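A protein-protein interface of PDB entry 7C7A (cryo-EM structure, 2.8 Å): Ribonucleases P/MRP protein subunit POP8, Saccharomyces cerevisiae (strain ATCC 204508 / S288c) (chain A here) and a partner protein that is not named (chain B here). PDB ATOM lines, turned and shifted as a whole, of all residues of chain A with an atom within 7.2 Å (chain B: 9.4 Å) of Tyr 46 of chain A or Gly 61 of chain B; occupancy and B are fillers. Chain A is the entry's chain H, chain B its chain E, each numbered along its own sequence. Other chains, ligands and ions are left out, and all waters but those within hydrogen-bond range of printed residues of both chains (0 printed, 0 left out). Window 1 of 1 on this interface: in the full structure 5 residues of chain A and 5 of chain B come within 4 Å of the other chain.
N of Ile 48 of chain A lies within hydrogen-bond range of O of Asn 59 of chain B, 3.3 Å away.
The backbone carbonyl oxygen (O) of Leu 60 of chain B lies within hydrogen-bond range of the backbone NH (N) of Gly 47 of chain A, 2.5 Å away.
The side-chain hydroxyl (OG) of Ser 55 of chain B lies within hydrogen-bond range of the side-chain amide nitrogen (ND2) of Asn 59 of chain B (3.1 Å).
The backbone carbonyl oxygen (O) of Ala 41 of chain A lies within hydrogen-bond range of the side-chain hydroxyl (OG) of Ser 45 of chain A, at 2.9 Å.
OH of Tyr 46 of chain A is in hydrogen-bond range of OG of Ser 79 of chain A (3.0 Å).
OG1 of Thr 83 of chain A lies within hydrogen-bond range of O of Ser 79 of chain A (2.7 Å).
O of Ser 45 of chain A touches N of Asp 62 of chain B, 3.5 Å away.
Tyr 63 of chain B touches Ser 45 of chain A.
Tyr 46 of chain A touches Leu 60 of chain B (C to O, 3.6 Å).
Gly 61 of chain B touches Tyr 46 of chain A.
Asn 59 of chain B touches Gly 47 of chain A.
Gly 47 of chain A touches Gly 61 of chain B.
Thr 83 of chain A touches Tyr 63 of chain B.
Printed residues of chain B within 4 Å of Ser 45 of chain A: Asp 62 and Tyr 63.
Tyr 46 of chain A touches just these residues of chain B: Leu 60 (3.6 Å) and Gly 61 (3.8 Å).
Thr 76 of chain A touches none of the printed residues of chain B.
Of the printed residues of chain B, Thr 83 of chain A touches Tyr 63 (3.3 Å).
Printed residues of chain A within 4 Å of Asn 59 of chain B: Gly 47 (3.7 Å) and Ile 48 (3.3 Å).
Printed residues of chain A within 4 Å of Leu 60 of chain B: Tyr 46 (3.6 Å) and Gly 47 (2.5 Å).
Of chain A, only Tyr 46 and Gly 47 come within 4 Å of Gly 61 of chain B.
Printed residues of chain A within 4 Å of Asp 62 of chain B: Ser 45.
Of the printed residues of chain A, Tyr 63 of chain B touches Ser 45 and Thr 83.
The nearest residue of chain B that does not touch Tyr 46 of chain A is Tyr 63 of chain B (4.2 Å).
The nearest printed residue of chain B that does not touch Ile 48 of chain A is Leu 58 of chain B (4.5 Å).
Of the 20 printed residues of chain B, 5 touch a printed residue of chain A.
Among the printed residues, 9 pairs touch across the chains.
Among the printed residues, no Asp or Glu carboxylate lies within 4 Å of a Lys or Arg side-chain nitrogen of the other chain.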
ATOM      1  N   ASN A  40      -7.303   6.917  13.055  1.00  0.00           N
ATOM      2  CA  ASN A  40      -7.445   8.305  12.637  1.00  0.00           C
ATOM      3  C   ASN A  40      -7.187   8.487  11.150  1.00  0.00           C
ATOM      4  O   ASN A  40      -7.911   9.241  10.490  1.00  0.00           O
ATOM      5  CB  ASN A  40      -6.492   9.197  13.436  1.00  0.00           C
ATOM      6  CG  ASN A  40      -6.864  10.666  13.362  1.00  0.00           C
ATOM      7  OD1 ASN A  40      -7.875  11.034  12.764  1.00  0.00           O
ATOM      8  ND2 ASN A  40      -6.043  11.515  13.970  1.00  0.00           N
ATOM      9  N   ALA A  41      -6.184   7.796  10.605  1.00  0.00           N
ATOM     10  CA  ALA A  41      -5.877   7.904   9.183  1.00  0.00           C
ATOM     11  C   ALA A  41      -7.031   7.390   8.333  1.00  0.00           C
ATOM     12  O   ALA A  41      -7.421   8.022   7.343  1.00  0.00           O
ATOM     13  CB  ALA A  41      -4.592   7.136   8.867  1.00  0.00           C
ATOM     14  N   LEU A  42      -7.588   6.236   8.703  1.00  0.00           N
ATOM     15  CA  LEU A  42      -8.668   5.633   7.932  1.00  0.00           C
ATOM     16  C   LEU A  42      -9.915   6.509   7.942  1.00  0.00           C
ATOM     17  O   LEU A  42     -10.608   6.620   6.927  1.00  0.00           O
ATOM     18  CB  LEU A  42      -8.994   4.239   8.471  1.00  0.00           C
ATOM     19  CG  LEU A  42      -7.875   3.207   8.307  1.00  0.00           C
ATOM     20  CD1 LEU A  42      -8.192   1.921   9.055  1.00  0.00           C
ATOM     21  CD2 LEU A  42      -7.613   2.926   6.835  1.00  0.00           C
ATOM     22  N   LYS A  43     -10.209   7.136   9.081  1.00  0.00           N
ATOM     23  CA  LYS A  43     -11.399   7.970   9.199  1.00  0.00           C
ATOM     24  C   LYS A  43     -11.184   9.339   8.564  1.00  0.00           C
ATOM     25  O   LYS A  43     -12.148   9.992   8.153  1.00  0.00           O
ATOM     26  CB  LYS A  43     -11.816   8.118  10.664  1.00  0.00           C
ATOM     27  CG  LYS A  43     -10.916   9.000  11.508  1.00  0.00           C
ATOM     28  CD  LYS A  43     -11.386   9.012  12.951  1.00  0.00           C
ATOM     29  CE  LYS A  43     -12.741   9.687  13.084  1.00  0.00           C
ATOM     30  NZ  LYS A  43     -12.687  11.132  12.731  1.00  0.00           N
ATOM     31  N   ARG A  44      -9.930   9.792   8.488  1.00  0.00           N
ATOM     32  CA  ARG A  44      -9.650  11.078   7.857  1.00  0.00           C
ATOM     33  C   ARG A  44      -9.647  10.963   6.338  1.00  0.00           C
ATOM     34  O   ARG A  44     -10.246  11.791   5.645  1.00  0.00           O
ATOM     35  CB  ARG A  44      -8.313  11.630   8.351  1.00  0.00           C
ATOM     36  CG  ARG A  44      -7.899  12.932   7.681  1.00  0.00           C
ATOM     37  CD  ARG A  44      -8.701  14.115   8.201  1.00  0.00           C
ATOM     38  NE  ARG A  44      -8.459  14.356   9.621  1.00  0.00           N
ATOM     39  CZ  ARG A  44      -7.413  15.025  10.097  1.00  0.00           C
ATOM     40  NH1 ARG A  44      -6.504  15.519   9.268  1.00  0.00           N
ATOM     41  NH2 ARG A  44      -7.273  15.198  11.404  1.00  0.00           N
ATOM     42  N   SER A  45      -8.980   9.941   5.803  1.00  0.00           N
ATOM     43  CA  SER A  45      -8.908   9.746   4.361  1.00  0.00           C
ATOM     44  C   SER A  45     -10.154   9.098   3.779  1.00  0.00           C
ATOM     45  O   SER A  45     -10.532   9.415   2.647  1.00  0.00           O
ATOM     46  CB  SER A  45      -7.688   8.894   4.000  1.00  0.00           C
ATOM     47  OG  SER A  45      -7.813   7.575   4.507  1.00  0.00           O
ATOM     48  N   TYR A  46     -10.797   8.200   4.520  1.00  0.00           N
ATOM     49  CA  TYR A  46     -11.986   7.498   4.062  1.00  0.00           C
ATOM     50  C   TYR A  46     -13.093   7.642   5.095  1.00  0.00           C
ATOM     51  O   TYR A  46     -12.881   8.179   6.187  1.00  0.00           O
ATOM     52  CB  TYR A  46     -11.700   6.008   3.819  1.00  0.00           C
ATOM     53  CG  TYR A  46     -10.975   5.696   2.526  1.00  0.00           C
ATOM     54  CD1 TYR A  46     -11.558   4.887   1.560  1.00  0.00           C
ATOM     55  CD2 TYR A  46      -9.703   6.198   2.277  1.00  0.00           C
ATOM     56  CE1 TYR A  46     -10.899   4.592   0.381  1.00  0.00           C
ATOM     57  CE2 TYR A  46      -9.037   5.910   1.101  1.00  0.00           C
ATOM     58  CZ  TYR A  46      -9.640   5.107   0.157  1.00  0.00           C
ATOM     59  OH  TYR A  46      -8.979   4.817  -1.017  1.00  0.00           O
ATOM     60  N   GLY A  47     -14.282   7.168   4.738  1.00  0.00           N
ATOM     61  CA  GLY A  47     -15.385   7.135   5.677  1.00  0.00           C
ATOM     62  C   GLY A  47     -15.449   5.818   6.420  1.00  0.00           C
ATOM     63  O   GLY A  47     -14.426   5.324   6.905  1.00  0.00           O
ATOM     64  N   ILE A  48     -16.645   5.234   6.512  1.00  0.00           N
ATOM     65  CA  ILE A  48     -16.787   3.922   7.135  1.00  0.00           C
ATOM     66  C   ILE A  48     -16.098   2.851   6.296  1.00  0.00           C
ATOM     67  O   ILE A  48     -15.699   1.801   6.814  1.00  0.00           O
ATOM     68  CB  ILE A  48     -18.276   3.601   7.356  1.00  0.00           C
ATOM     69  CG1 ILE A  48     -19.045   4.866   7.746  1.00  0.00           C
ATOM     70  CG2 ILE A  48     -18.443   2.527   8.420  1.00  0.00           C
ATOM     71  CD1 ILE A  48     -18.655   5.434   9.097  1.00  0.00           C
ATOM     72  N   PHE A  49     -15.953   3.103   4.993  1.00  0.00           N
ATOM     73  CA  PHE A  49     -15.271   2.161   4.112  1.00  0.00           C
ATOM     74  C   PHE A  49     -13.851   1.891   4.594  1.00  0.00           C
ATOM     75  O   PHE A  49     -13.432   0.734   4.716  1.00  0.00           O
ATOM     76  CB  PHE A  49     -15.267   2.701   2.679  1.00  0.00           C
ATOM     77  CG  PHE A  49     -14.719   1.737   1.662  1.00  0.00           C
ATOM     78  CD1 PHE A  49     -13.364   1.713   1.365  1.00  0.00           C
ATOM     79  CD2 PHE A  49     -15.561   0.865   0.992  1.00  0.00           C
ATOM     80  CE1 PHE A  49     -12.861   0.831   0.428  1.00  0.00           C
ATOM     81  CE2 PHE A  49     -15.063  -0.020   0.054  1.00  0.00           C
ATOM     82  CZ  PHE A  49     -13.711  -0.037  -0.229  1.00  0.00           C
ATOM     83  N   GLY A  50     -13.093   2.952   4.874  1.00  0.00           N
ATOM     84  CA  GLY A  50     -11.743   2.770   5.378  1.00  0.00           C
ATOM     85  C   GLY A  50     -11.703   2.304   6.819  1.00  0.00           C
ATOM     86  O   GLY A  50     -10.775   1.598   7.221  1.00  0.00           O
ATOM     87  N   GLU A  51     -12.704   2.684   7.616  1.00  0.00           N
ATOM     88  CA  GLU A  51     -12.741   2.283   9.016  1.00  0.00           C
ATOM     89  C   GLU A  51     -13.036   0.802   9.197  1.00  0.00           C
ATOM     90  O   GLU A  51     -12.612   0.218  10.202  1.00  0.00           O
ATOM     91  CB  GLU A  51     -13.784   3.107   9.776  1.00  0.00           C
ATOM     92  CG  GLU A  51     -13.460   4.588   9.877  1.00  0.00           C
ATOM     93  CD  GLU A  51     -14.297   5.296  10.924  1.00  0.00           C
ATOM     94  OE1 GLU A  51     -14.596   6.494  10.739  1.00  0.00           O
ATOM     95  OE2 GLU A  51     -14.648   4.655  11.935  1.00  0.00           O
ATOM     96  N   VAL A  53     -11.802  -1.642   7.635  1.00  0.00           N
ATOM     97  CA  VAL A  53     -10.718  -2.460   7.106  1.00  0.00           C
ATOM     98  C   VAL A  53     -10.131  -3.306   8.228  1.00  0.00           C
ATOM     99  O   VAL A  53      -9.842  -2.803   9.322  1.00  0.00           O
ATOM    100  CB  VAL A  53      -9.647  -1.577   6.449  1.00  0.00           C
ATOM    101  CG1 VAL A  53      -8.395  -2.386   6.143  1.00  0.00           C
ATOM    102  CG2 VAL A  53     -10.194  -0.937   5.181  1.00  0.00           C
ATOM    103  N   ASP A  75      -5.223  -2.287  -1.840  1.00  0.00           N
ATOM    104  CA  ASP A  75      -5.261  -0.979  -2.484  1.00  0.00           C
ATOM    105  C   ASP A  75      -5.778   0.100  -1.542  1.00  0.00           C
ATOM    106  O   ASP A  75      -5.194   1.188  -1.471  1.00  0.00           O
ATOM    107  CB  ASP A  75      -6.115  -1.052  -3.752  1.00  0.00           C
ATOM    108  CG  ASP A  75      -7.541  -1.510  -3.476  1.00  0.00           C
ATOM    109  OD1 ASP A  75      -7.867  -1.821  -2.312  1.00  0.00           O
ATOM    110  OD2 ASP A  75      -8.338  -1.567  -4.434  1.00  0.00           O
ATOM    111  N   THR A  76      -6.857  -0.184  -0.807  1.00  0.00           N
ATOM    112  CA  THR A  76      -7.376   0.775   0.162  1.00  0.00           C
ATOM    113  C   THR A  76      -6.349   1.070   1.251  1.00  0.00           C
ATOM    114  O   THR A  76      -6.223   2.214   1.706  1.00  0.00           O
ATOM    115  CB  THR A  76      -8.679   0.251   0.775  1.00  0.00           C
ATOM    116  OG1 THR A  76      -9.671   0.108  -0.251  1.00  0.00           O
ATOM    117  CG2 THR A  76      -9.202   1.200   1.846  1.00  0.00           C
ATOM    118  N   PHE A  77      -5.593   0.053   1.671  1.00  0.00           N
ATOM    119  CA  PHE A  77      -4.603   0.260   2.723  1.00  0.00           C
ATOM    120  C   PHE A  77      -3.418   1.075   2.216  1.00  0.00           C
ATOM    121  O   PHE A  77      -2.965   2.007   2.891  1.00  0.00           O
ATOM    122  CB  PHE A  77      -4.135  -1.087   3.277  1.00  0.00           C
ATOM    123  CG  PHE A  77      -3.200  -0.973   4.451  1.00  0.00           C
ATOM    124  CD1 PHE A  77      -3.683  -0.652   5.710  1.00  0.00           C
ATOM    125  CD2 PHE A  77      -1.842  -1.195   4.299  1.00  0.00           C
ATOM    126  CE1 PHE A  77      -2.827  -0.550   6.793  1.00  0.00           C
ATOM    127  CE2 PHE A  77      -0.981  -1.095   5.377  1.00  0.00           C
ATOM    128  CZ  PHE A  77      -1.476  -0.772   6.625  1.00  0.00           C
ATOM    129  N   SER A  79      -3.335   3.121  -0.331  1.00  0.00           N
ATOM    130  CA  SER A  79      -3.703   4.483  -0.689  1.00  0.00           C
ATOM    131  C   SER A  79      -3.912   5.355   0.541  1.00  0.00           C
ATOM    132  O   SER A  79      -3.734   6.577   0.470  1.00  0.00           O
ATOM    133  CB  SER A  79      -4.971   4.478  -1.542  1.00  0.00           C
ATOM    134  OG  SER A  79      -6.076   4.006  -0.790  1.00  0.00           O
ATOM    135  N   SER A  80      -4.298   4.752   1.667  1.00  0.00           N
ATOM    136  CA  SER A  80      -4.511   5.516   2.889  1.00  0.00           C
ATOM    137  C   SER A  80      -3.222   5.717   3.678  1.00  0.00           C
ATOM    138  O   SER A  80      -3.067   6.746   4.347  1.00  0.00           O
ATOM    139  CB  SER A  80      -5.558   4.822   3.764  1.00  0.00           C
ATOM    140  OG  SER A  80      -5.090   3.565   4.221  1.00  0.00           O
ATOM    141  N   THR A  83      -1.028   8.601   2.371  1.00  0.00           N
ATOM    142  CA  THR A  83      -1.739   9.865   2.260  1.00  0.00           C
ATOM    143  C   THR A  83      -1.682  10.589   3.593  1.00  0.00           C
ATOM    144  O   THR A  83      -1.212  11.743   3.652  1.00  0.00           O
ATOM    145  CB  THR A  83      -3.177   9.632   1.776  1.00  0.00           C
ATOM    146  OG1 THR A  83      -3.162   9.182   0.415  1.00  0.00           O
ATOM    147  CG2 THR A  83      -3.985  10.915   1.877  1.00  0.00           C
ATOM    148  N   ILE B  52     -27.397  14.730  -1.301  1.00  0.00           N
ATOM    149  CA  ILE B  52     -26.666  13.559  -1.774  1.00  0.00           C
ATOM    150  C   ILE B  52     -25.163  13.802  -1.719  1.00  0.00           C
ATOM    151  O   ILE B  52     -24.391  12.875  -1.450  1.00  0.00           O
ATOM    152  CB  ILE B  52     -27.140  13.148  -3.186  1.00  0.00           C
ATOM    153  CG1 ILE B  52     -26.728  11.706  -3.489  1.00  0.00           C
ATOM    154  CG2 ILE B  52     -26.602  14.086  -4.255  1.00  0.00           C
ATOM    155  CD1 ILE B  52     -27.157  11.223  -4.857  1.00  0.00           C
ATOM    156  N   ARG B  53     -24.722  15.047  -1.927  1.00  0.00           N
ATOM    157  CA  ARG B  53     -23.306  15.365  -1.787  1.00  0.00           C
ATOM    158  C   ARG B  53     -22.837  15.235  -0.345  1.00  0.00           C
ATOM    159  O   ARG B  53     -21.720  14.767  -0.101  1.00  0.00           O
ATOM    160  CB  ARG B  53     -23.029  16.780  -2.296  1.00  0.00           C
ATOM    161  CG  ARG B  53     -22.860  16.887  -3.802  1.00  0.00           C
ATOM    162  CD  ARG B  53     -22.703  18.338  -4.229  1.00  0.00           C
ATOM    163  NE  ARG B  53     -22.369  18.463  -5.645  1.00  0.00           N
ATOM    164  CZ  ARG B  53     -22.208  19.623  -6.274  1.00  0.00           C
ATOM    165  NH1 ARG B  53     -22.348  20.763  -5.612  1.00  0.00           N
ATOM    166  NH2 ARG B  53     -21.904  19.643  -7.564  1.00  0.00           N
ATOM    167  N   ARG B  54     -23.669  15.645   0.613  1.00  0.00           N
ATOM    168  CA  ARG B  54     -23.331  15.472   2.022  1.00  0.00           C
ATOM    169  C   ARG B  54     -23.286  13.994   2.395  1.00  0.00           C
ATOM    170  O   ARG B  54     -22.365  13.544   3.086  1.00  0.00           O
ATOM    171  CB  ARG B  54     -24.340  16.220   2.899  1.00  0.00           C
ATOM    172  CG  ARG B  54     -23.886  16.429   4.335  1.00  0.00           C
ATOM    173  CD  ARG B  54     -24.931  17.191   5.136  1.00  0.00           C
ATOM    174  NE  ARG B  54     -25.390  18.390   4.442  1.00  0.00           N
ATOM    175  CZ  ARG B  54     -26.365  19.181   4.880  1.00  0.00           C
ATOM    176  NH1 ARG B  54     -26.989  18.902   6.016  1.00  0.00           N
ATOM    177  NH2 ARG B  54     -26.716  20.252   4.182  1.00  0.00           N
ATOM    178  N   SER B  55     -24.276  13.223   1.936  1.00  0.00           N
ATOM    179  CA  SER B  55     -24.324  11.801   2.267  1.00  0.00           C
ATOM    180  C   SER B  55     -23.160  11.043   1.641  1.00  0.00           C
ATOM    181  O   SER B  55     -22.628  10.100   2.238  1.00  0.00           O
ATOM    182  CB  SER B  55     -25.658  11.204   1.817  1.00  0.00           C
ATOM    183  OG  SER B  55     -25.719   9.817   2.103  1.00  0.00           O
ATOM    184  N   LEU B  56     -22.745  11.449   0.438  1.00  0.00           N
ATOM    185  CA  LEU B  56     -21.611  10.805  -0.213  1.00  0.00           C
ATOM    186  C   LEU B  56     -20.336  10.990   0.598  1.00  0.00           C
ATOM    187  O   LEU B  56     -19.583  10.034   0.814  1.00  0.00           O
ATOM    188  CB  LEU B  56     -21.439  11.373  -1.622  1.00  0.00           C
ATOM    189  CG  LEU B  56     -20.568  10.601  -2.610  1.00  0.00           C
ATOM    190  CD1 LEU B  56     -21.315   9.391  -3.148  1.00  0.00           C
ATOM    191  CD2 LEU B  56     -20.135  11.519  -3.739  1.00  0.00           C
ATOM    192  N   SER B  57     -20.083  12.215   1.065  1.00  0.00           N
ATOM    193  CA  SER B  57     -18.903  12.469   1.882  1.00  0.00           C
ATOM    194  C   SER B  57     -19.012  11.785   3.239  1.00  0.00           C
ATOM    195  O   SER B  57     -18.006  11.325   3.793  1.00  0.00           O
ATOM    196  CB  SER B  57     -18.695  13.974   2.051  1.00  0.00           C
ATOM    197  OG  SER B  57     -19.742  14.557   2.809  1.00  0.00           O
ATOM    198  N   LEU B  58     -20.222  11.704   3.790  1.00  0.00           N
ATOM    199  CA  LEU B  58     -20.437  11.091   5.095  1.00  0.00           C
ATOM    200  C   LEU B  58     -20.293   9.574   5.074  1.00  0.00           C
ATOM    201  O   LEU B  58     -19.887   8.994   6.087  1.00  0.00           O
ATOM    202  CB  LEU B  58     -21.824  11.472   5.620  1.00  0.00           C
ATOM    203  CG  LEU B  58     -22.182  11.069   7.051  1.00  0.00           C
ATOM    204  CD1 LEU B  58     -21.247  11.745   8.038  1.00  0.00           C
ATOM    205  CD2 LEU B  58     -23.634  11.409   7.360  1.00  0.00           C
ATOM    206  N   ASN B  59     -20.607   8.917   3.953  1.00  0.00           N
ATOM    207  CA  ASN B  59     -20.553   7.466   3.884  1.00  0.00           C
ATOM    208  C   ASN B  59     -19.223   7.058   3.291  1.00  0.00           C
ATOM    209  O   ASN B  59     -18.473   6.282   3.921  1.00  0.00           O
ATOM    210  CB  ASN B  59     -21.761   6.929   3.100  1.00  0.00           C
ATOM    211  CG  ASN B  59     -23.060   7.059   3.869  1.00  0.00           C
ATOM    212  OD1 ASN B  59     -23.101   6.847   5.080  1.00  0.00           O
ATOM    213  ND2 ASN B  59     -24.132   7.407   3.165  1.00  0.00           N
ATOM    214  N   LEU B  60     -18.858   7.532   2.097  1.00  0.00           N
ATOM    215  CA  LEU B  60     -17.627   7.079   1.457  1.00  0.00           C
ATOM    216  C   LEU B  60     -16.403   7.723   2.095  1.00  0.00           C
ATOM    217  O   LEU B  60     -15.468   7.033   2.518  1.00  0.00           O
ATOM    218  CB  LEU B  60     -17.682   7.380  -0.040  1.00  0.00           C
ATOM    219  CG  LEU B  60     -18.694   6.550  -0.830  1.00  0.00           C
ATOM    220  CD1 LEU B  60     -18.734   7.006  -2.271  1.00  0.00           C
ATOM    221  CD2 LEU B  60     -18.344   5.073  -0.749  1.00  0.00           C
ATOM    222  N   GLY B  61     -16.383   9.052   2.159  1.00  0.00           N
ATOM    223  CA  GLY B  61     -15.256   9.762   2.730  1.00  0.00           C
ATOM    224  C   GLY B  61     -14.814  10.951   1.901  1.00  0.00           C
ATOM    225  O   GLY B  61     -15.648  11.667   1.339  1.00  0.00           O
ATOM    226  N   ASP B  62     -13.502  11.169   1.813  1.00  0.00           N
ATOM    227  CA  ASP B  62     -12.957  12.308   1.065  1.00  0.00           C
ATOM    228  C   ASP B  62     -12.672  11.915  -0.382  1.00  0.00           C
ATOM    229  O   ASP B  62     -13.167  12.551  -1.317  1.00  0.00           O
ATOM    230  CB  ASP B  62     -11.701  12.842   1.755  1.00  0.00           C
ATOM    231  CG  ASP B  62     -11.268  14.189   1.214  1.00  0.00           C
ATOM    232  OD1 ASP B  62     -12.074  14.834   0.510  1.00  0.00           O
ATOM    233  OD2 ASP B  62     -10.122  14.604   1.490  1.00  0.00           O
ATOM    234  N   TYR B  63     -11.870  10.866  -0.577  1.00  0.00           N
ATOM    235  CA  TYR B  63     -11.539  10.423  -1.926  1.00  0.00           C
ATOM    236  C   TYR B  63     -12.753   9.813  -2.617  1.00  0.00           C
ATOM    237  O   TYR B  63     -12.921   9.933  -3.836  1.00  0.00           O
ATOM    238  CB  TYR B  63     -10.377   9.427  -1.878  1.00  0.00           C
ATOM    239  CG  TYR B  63      -9.036  10.076  -1.622  1.00  0.00           C
ATOM    240  CD1 TYR B  63      -8.848  11.436  -1.838  1.00  0.00           C
ATOM    241  CD2 TYR B  63      -7.958   9.332  -1.162  1.00  0.00           C
ATOM    242  CE1 TYR B  63      -7.624  12.035  -1.604  1.00  0.00           C
ATOM    243  CE2 TYR B  63      -6.730   9.923  -0.925  1.00  0.00           C
ATOM    244  CZ  TYR B  63      -6.569  11.275  -1.147  1.00  0.00           C
ATOM    245  OH  TYR B  63      -5.351  11.870  -0.915  1.00  0.00           O
ATOM    246  N   GLY B  64     -13.615   9.147  -1.845  1.00  0.00           N
ATOM    247  CA  GLY B  64     -14.847   8.614  -2.400  1.00  0.00           C
ATOM    248  C   GLY B  64     -15.783   9.680  -2.928  1.00  0.00           C
ATOM    249  O   GLY B  64     -16.527   9.424  -3.881  1.00  0.00           O
ATOM    250  N   SER B  65     -15.765  10.870  -2.327  1.00  0.00           N
ATOM    251  CA  SER B  65     -16.558  11.981  -2.840  1.00  0.00           C
ATOM    252  C   SER B  65     -15.820  12.711  -3.953  1.00  0.00           C
ATOM    253  O   SER B  65     -16.442  13.244  -4.878  1.00  0.00           O
ATOM    254  CB  SER B  65     -16.911  12.944  -1.706  1.00  0.00           C
ATOM    255  OG  SER B  65     -17.676  14.035  -2.188  1.00  0.00           O
ATOM    256  N   ALA B  66     -14.486  12.736  -3.883  1.00  0.00           N
ATOM    257  CA  ALA B  66     -13.700  13.420  -4.901  1.00  0.00           C
ATOM    258  C   ALA B  66     -13.769  12.703  -6.243  1.00  0.00           C
ATOM    259  O   ALA B  66     -13.892  13.351  -7.287  1.00  0.00           O
ATOM    260  CB  ALA B  66     -12.247  13.544  -4.441  1.00  0.00           C
ATOM    261  N   LYS B  67     -13.692  11.371  -6.236  1.00  0.00           N
ATOM    262  CA  LYS B  67     -13.775  10.623  -7.484  1.00  0.00           C
ATOM    263  C   LYS B  67     -15.190  10.621  -8.046  1.00  0.00           C
ATOM    264  O   LYS B  67     -15.370  10.496  -9.262  1.00  0.00           O
ATOM    265  CB  LYS B  67     -13.288   9.189  -7.271  1.00  0.00           C
ATOM    266  CG  LYS B  67     -11.784   9.062  -7.078  1.00  0.00           C
ATOM    267  CD  LYS B  67     -11.416   7.753  -6.391  1.00  0.00           C
ATOM    268  CE  LYS B  67     -11.431   6.590  -7.370  1.00  0.00           C
ATOM    269  NZ  LYS B  67     -10.724   5.399  -6.829  1.00  0.00           N
ATOM    270  N   CYS B  68     -16.201  10.771  -7.186  1.00  0.00           N
ATOM    271  CA  CYS B  68     -17.586  10.650  -7.630  1.00  0.00           C
ATOM    272  C   CYS B  68     -18.174  11.992  -8.054  1.00  0.00           C
ATOM    273  O   CYS B  68     -19.063  12.036  -8.911  1.00  0.00           O
ATOM    274  CB  CYS B  68     -18.433  10.026  -6.520  1.00  0.00           C
ATOM    275  SG  CYS B  68     -20.167   9.769  -6.951  1.00  0.00           S
ATOM    276  N   ASN B  69     -17.693  13.092  -7.474  1.00  0.00           N
ATOM    277  CA  ASN B  69     -18.239  14.416  -7.733  1.00  0.00           C
ATOM    278  C   ASN B  69     -17.660  15.063  -8.988  1.00  0.00           C
ATOM    279  O   ASN B  69     -17.766  16.284  -9.149  1.00  0.00           O
ATOM    280  CB  ASN B  69     -18.008  15.322  -6.522  1.00  0.00           C
ATOM    281  CG  ASN B  69     -19.092  16.366  -6.359  1.00  0.00           C
ATOM    282  OD1 ASN B  69     -20.177  16.246  -6.929  1.00  0.00           O
ATOM    283  ND2 ASN B  69     -18.805  17.401  -5.578  1.00  0.00           N
ATOM    284  N   LEU B  95     -21.197   3.569  -6.762  1.00  0.00           N
ATOM    285  CA  LEU B  95     -21.080   4.514  -5.656  1.00  0.00           C
ATOM    286  C   LEU B  95     -22.341   5.357  -5.516  1.00  0.00           C
ATOM    287  O   LEU B  95     -22.863   5.527  -4.407  1.00  0.00           O
ATOM    288  CB  LEU B  95     -19.857   5.410  -5.861  1.00  0.00           C
ATOM    289  CG  LEU B  95     -18.461   4.844  -5.573  1.00  0.00           C
ATOM    290  CD1 LEU B  95     -18.018   3.869  -6.654  1.00  0.00           C
ATOM    291  CD2 LEU B  95     -17.450   5.971  -5.440  1.00  0.00           C
ATOM    292  N   MET B  98     -25.206   3.164  -4.187  1.00  0.00           N
ATOM    293  CA  MET B  98     -25.084   2.910  -2.756  1.00  0.00           C
ATOM    294  C   MET B  98     -25.379   4.161  -1.937  1.00  0.00           C
ATOM    295  O   MET B  98     -25.955   4.065  -0.847  1.00  0.00           O
ATOM    296  CB  MET B  98     -23.687   2.379  -2.430  1.00  0.00           C
ATOM    297  CG  MET B  98     -23.590   1.691  -1.076  1.00  0.00           C
ATOM    298  SD  MET B  98     -21.926   1.115  -0.691  1.00  0.00           S
ATOM    299  CE  MET B  98     -21.074   2.676  -0.492  1.00  0.00           C
